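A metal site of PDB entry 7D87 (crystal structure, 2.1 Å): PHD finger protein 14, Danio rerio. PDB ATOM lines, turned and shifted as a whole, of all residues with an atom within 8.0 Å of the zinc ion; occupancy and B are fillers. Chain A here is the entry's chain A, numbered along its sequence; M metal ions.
N of Ala 150 sits close to SG of Cys 148 (3.4 Å). The side-chain sulfur (SG) of Cys 185 sits close to the backbone NH (N) of Gln 187 (3.5 Å). The backbone carbonyl oxygen of Ser 155 lies within hydrogen-bond range of the backbone NH of Cys 148 (2.9 Å).
The zinc ion is bound by ND1 of His 188 (2.1 Å), SG of Cys 185 (2.3 Å), SG of Cys 148 (2.3 Å) and SG of Cys 153 (2.3 Å).
Four residues have an atom within 4 Å of the zinc ion: Cys 148, Cys 153, Cys 185 and His 188.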
ATOM      1  N   SER A 147      11.051  -3.019 -23.375  1.00  0.00           N
ATOM      2  CA  SER A 147      10.043  -3.195 -22.354  1.00  0.00           C
ATOM      3  C   SER A 147      10.621  -2.924 -20.972  1.00  0.00           C
ATOM      4  O   SER A 147      11.832  -2.921 -20.766  1.00  0.00           O
ATOM      5  CB  SER A 147       9.429  -4.588 -22.403  1.00  0.00           C
ATOM      6  OG  SER A 147      10.419  -5.553 -22.110  1.00  0.00           O
ATOM      7  N   CYS A 148       9.723  -2.678 -20.024  1.00  0.00           N
ATOM      8  CA  CYS A 148      10.073  -2.694 -18.609  1.00  0.00           C
ATOM      9  C   CYS A 148      10.771  -3.998 -18.263  1.00  0.00           C
ATOM     10  O   CYS A 148      10.347  -5.077 -18.699  1.00  0.00           O
ATOM     11  CB  CYS A 148       8.809  -2.506 -17.764  1.00  0.00           C
ATOM     12  SG  CYS A 148       9.062  -2.652 -15.984  1.00  0.00           S
ATOM     13  N   ASP A 149      11.833  -3.914 -17.471  1.00  0.00           N
ATOM     14  CA  ASP A 149      12.583  -5.104 -17.077  1.00  0.00           C
ATOM     15  C   ASP A 149      12.185  -5.664 -15.716  1.00  0.00           C
ATOM     16  O   ASP A 149      12.894  -6.531 -15.199  1.00  0.00           O
ATOM     17  CB  ASP A 149      14.087  -4.775 -17.068  1.00  0.00           C
ATOM     18  CG  ASP A 149      14.670  -4.718 -18.497  1.00  0.00           C
ATOM     19  OD1 ASP A 149      14.387  -5.648 -19.282  1.00  0.00           O
ATOM     20  OD2 ASP A 149      15.349  -3.728 -18.839  1.00  0.00           O
ATOM     21  N   ALA A 150      11.076  -5.208 -15.127  1.00  0.00           N
ATOM     22  CA  ALA A 150      10.636  -5.694 -13.820  1.00  0.00           C
ATOM     23  C   ALA A 150       9.785  -6.953 -14.010  1.00  0.00           C
ATOM     24  O   ALA A 150       8.716  -6.878 -14.618  1.00  0.00           O
ATOM     25  CB  ALA A 150       9.843  -4.625 -13.076  1.00  0.00           C
ATOM     26  N   GLY A 151      10.248  -8.078 -13.475  1.00  0.00           N
ATOM     27  CA  GLY A 151       9.536  -9.338 -13.656  1.00  0.00           C
ATOM     28  C   GLY A 151       9.045  -9.585 -15.067  1.00  0.00           C
ATOM     29  O   GLY A 151       9.831  -9.559 -16.018  1.00  0.00           O
ATOM     30  N   MET A 152       7.734  -9.799 -15.212  1.00  0.00           N
ATOM     31  CA  MET A 152       7.118 -10.081 -16.499  1.00  0.00           C
ATOM     32  C   MET A 152       6.308  -8.893 -17.032  1.00  0.00           C
ATOM     33  O   MET A 152       5.389  -9.091 -17.815  1.00  0.00           O
ATOM     34  CB  MET A 152       6.225 -11.310 -16.394  1.00  0.00           C
ATOM     35  CG  MET A 152       6.948 -12.560 -15.946  1.00  0.00           C
ATOM     36  SD  MET A 152       8.138 -13.141 -17.170  1.00  0.00           S
ATOM     37  CE  MET A 152       9.668 -12.769 -16.348  1.00  0.00           C
ATOM     38  N   CYS A 153       6.625  -7.678 -16.593  1.00  0.00           N
ATOM     39  CA  CYS A 153       5.873  -6.496 -17.008  1.00  0.00           C
ATOM     40  C   CYS A 153       6.017  -6.256 -18.504  1.00  0.00           C
ATOM     41  O   CYS A 153       7.126  -6.166 -19.027  1.00  0.00           O
ATOM     42  CB  CYS A 153       6.361  -5.275 -16.218  1.00  0.00           C
ATOM     43  SG  CYS A 153       5.507  -3.724 -16.567  1.00  0.00           S
ATOM     44  N   ARG A 154       4.886  -6.143 -19.189  1.00  0.00           N
ATOM     45  CA  ARG A 154       4.894  -5.941 -20.641  1.00  0.00           C
ATOM     46  C   ARG A 154       4.482  -4.512 -20.976  1.00  0.00           C
ATOM     47  O   ARG A 154       3.537  -4.291 -21.732  1.00  0.00           O
ATOM     48  CB  ARG A 154       3.948  -6.952 -21.320  1.00  0.00           C
ATOM     49  CG  ARG A 154       4.321  -8.404 -21.088  1.00  0.00           C
ATOM     50  CD  ARG A 154       5.271  -8.906 -22.162  1.00  0.00           C
ATOM     51  NE  ARG A 154       6.607  -8.336 -22.043  1.00  0.00           N
ATOM     52  CZ  ARG A 154       7.540  -8.415 -22.988  1.00  0.00           C
ATOM     53  NH1 ARG A 154       8.726  -7.862 -22.793  1.00  0.00           N
ATOM     54  NH2 ARG A 154       7.275  -9.040 -24.124  1.00  0.00           N
ATOM     55  N   SER A 155       5.178  -3.540 -20.402  1.00  0.00           N
ATOM     56  CA  SER A 155       4.997  -2.137 -20.750  1.00  0.00           C
ATOM     57  C   SER A 155       6.102  -1.752 -21.730  1.00  0.00           C
ATOM     58  O   SER A 155       7.268  -2.017 -21.464  1.00  0.00           O
ATOM     59  CB  SER A 155       5.041  -1.261 -19.493  1.00  0.00           C
ATOM     60  OG  SER A 155       4.755   0.086 -19.796  1.00  0.00           O
ATOM     61  N   PHE A 156       5.726  -1.145 -22.863  1.00  0.00           N
ATOM     62  CA  PHE A 156       6.658  -0.913 -23.968  1.00  0.00           C
ATOM     63  C   PHE A 156       6.848   0.581 -24.243  1.00  0.00           C
ATOM     64  O   PHE A 156       5.921   1.388 -24.109  1.00  0.00           O
ATOM     65  CB  PHE A 156       6.187  -1.605 -25.274  1.00  0.00           C
ATOM     66  CG  PHE A 156       5.827  -3.072 -25.102  1.00  0.00           C
ATOM     67  CD1 PHE A 156       6.802  -3.996 -24.766  1.00  0.00           C
ATOM     68  CD2 PHE A 156       4.524  -3.505 -25.286  1.00  0.00           C
ATOM     69  CE1 PHE A 156       6.485  -5.331 -24.600  1.00  0.00           C
ATOM     70  CE2 PHE A 156       4.191  -4.839 -25.115  1.00  0.00           C
ATOM     71  CZ  PHE A 156       5.175  -5.753 -24.769  1.00  0.00           C
ATOM     72  N   PHE A 157       8.070   0.941 -24.645  1.00  0.00           N
ATOM     73  CA  PHE A 157       8.362   2.316 -25.003  1.00  0.00           C
ATOM     74  C   PHE A 157       9.646   2.391 -25.812  1.00  0.00           C
ATOM     75  O   PHE A 157      10.537   1.551 -25.671  1.00  0.00           O
ATOM     76  CB  PHE A 157       8.514   3.201 -23.757  1.00  0.00           C
ATOM     77  CG  PHE A 157       9.011   2.437 -22.543  1.00  0.00           C
ATOM     78  CD1 PHE A 157      10.291   1.926 -22.497  1.00  0.00           C
ATOM     79  CD2 PHE A 157       8.160   2.206 -21.469  1.00  0.00           C
ATOM     80  CE1 PHE A 157      10.729   1.200 -21.385  1.00  0.00           C
ATOM     81  CE2 PHE A 157       8.603   1.489 -20.360  1.00  0.00           C
ATOM     82  CZ  PHE A 157       9.880   0.988 -20.323  1.00  0.00           C
ATOM     83  N   ALA A 183      15.627  -0.855 -18.115  1.00  0.00           N
ATOM     84  CA  ALA A 183      14.608   0.171 -17.963  1.00  0.00           C
ATOM     85  C   ALA A 183      13.434  -0.392 -17.173  1.00  0.00           C
ATOM     86  O   ALA A 183      13.143  -1.595 -17.239  1.00  0.00           O
ATOM     87  CB  ALA A 183      14.112   0.676 -19.322  1.00  0.00           C
ATOM     88  N   TYR A 184      12.761   0.496 -16.435  1.00  0.00           N
ATOM     89  CA  TYR A 184      11.545   0.188 -15.707  1.00  0.00           C
ATOM     90  C   TYR A 184      10.473   1.179 -16.130  1.00  0.00           C
ATOM     91  O   TYR A 184      10.763   2.360 -16.344  1.00  0.00           O
ATOM     92  CB  TYR A 184      11.721   0.290 -14.191  1.00  0.00           C
ATOM     93  CG  TYR A 184      12.672  -0.712 -13.582  1.00  0.00           C
ATOM     94  CD1 TYR A 184      12.691  -2.044 -13.992  1.00  0.00           C
ATOM     95  CD2 TYR A 184      13.559  -0.327 -12.582  1.00  0.00           C
ATOM     96  CE1 TYR A 184      13.583  -2.955 -13.419  1.00  0.00           C
ATOM     97  CE2 TYR A 184      14.431  -1.228 -12.012  1.00  0.00           C
ATOM     98  CZ  TYR A 184      14.440  -2.533 -12.431  1.00  0.00           C
ATOM     99  OH  TYR A 184      15.307  -3.410 -11.841  1.00  0.00           O
ATOM    100  N   CYS A 185       9.232   0.707 -16.237  1.00  0.00           N
ATOM    101  CA  CYS A 185       8.144   1.646 -16.464  1.00  0.00           C
ATOM    102  C   CYS A 185       7.919   2.480 -15.204  1.00  0.00           C
ATOM    103  O   CYS A 185       8.510   2.234 -14.146  1.00  0.00           O
ATOM    104  CB  CYS A 185       6.880   0.902 -16.857  1.00  0.00           C
ATOM    105  SG  CYS A 185       6.152  -0.073 -15.497  1.00  0.00           S
ATOM    106  N   LYS A 186       7.051   3.484 -15.304  1.00  0.00           N
ATOM    107  CA  LYS A 186       6.833   4.371 -14.167  1.00  0.00           C
ATOM    108  C   LYS A 186       6.280   3.614 -12.982  1.00  0.00           C
ATOM    109  O   LYS A 186       6.565   3.978 -11.827  1.00  0.00           O
ATOM    110  CB  LYS A 186       5.890   5.503 -14.552  1.00  0.00           C
ATOM    111  CG  LYS A 186       6.385   6.376 -15.687  1.00  0.00           C
ATOM    112  CD  LYS A 186       5.318   7.424 -16.031  1.00  0.00           C
ATOM    113  CE  LYS A 186       5.540   8.001 -17.414  1.00  0.00           C
ATOM    114  NZ  LYS A 186       4.385   8.841 -17.872  1.00  0.00           N
ATOM    115  N   GLN A 187       5.496   2.558 -13.241  1.00  0.00           N
ATOM    116  CA  GLN A 187       4.902   1.797 -12.148  1.00  0.00           C
ATOM    117  C   GLN A 187       5.964   1.081 -11.327  1.00  0.00           C
ATOM    118  O   GLN A 187       5.798   0.885 -10.126  1.00  0.00           O
ATOM    119  CB  GLN A 187       3.888   0.800 -12.712  1.00  0.00           C
ATOM    120  CG  GLN A 187       3.166   0.001 -11.647  1.00  0.00           C
ATOM    121  CD  GLN A 187       2.227  -1.028 -12.247  1.00  0.00           C
ATOM    122  OE1 GLN A 187       2.020  -1.059 -13.466  1.00  0.00           O
ATOM    123  NE2 GLN A 187       1.659  -1.886 -11.397  1.00  0.00           N
ATOM    124  N   HIS A 188       7.091   0.751 -11.943  1.00  0.00           N
ATOM    125  CA  HIS A 188       8.101  -0.060 -11.298  1.00  0.00           C
ATOM    126  C   HIS A 188       9.417   0.671 -11.091  1.00  0.00           C
ATOM    127  O   HIS A 188      10.377   0.070 -10.596  1.00  0.00           O
ATOM    128  CB  HIS A 188       8.325  -1.331 -12.122  1.00  0.00           C
ATOM    129  CG  HIS A 188       7.138  -2.229 -12.148  1.00  0.00           C
ATOM    130  ND1 HIS A 188       6.580  -2.713 -13.313  1.00  0.00           N
ATOM    131  CD2 HIS A 188       6.370  -2.717 -11.134  1.00  0.00           C
ATOM    132  CE1 HIS A 188       5.518  -3.456 -13.019  1.00  0.00           C
ATOM    133  NE2 HIS A 188       5.373  -3.467 -11.704  1.00  0.00           N
ATOM    134  N   ALA A 189       9.488   1.945 -11.435  1.00  0.00           N
ATOM    135  CA  ALA A 189      10.750   2.655 -11.403  1.00  0.00           C
ATOM    136  C   ALA A 189      11.133   3.038  -9.989  1.00  0.00           C
ATOM    137  O   ALA A 189      10.303   3.085  -9.069  1.00  0.00           O
ATOM    138  CB  ALA A 189      10.677   3.907 -12.268  1.00  0.00           C
HETATM  139 ZN    ZN M   1       6.859  -2.249 -15.364  1.00  0.00          ZN
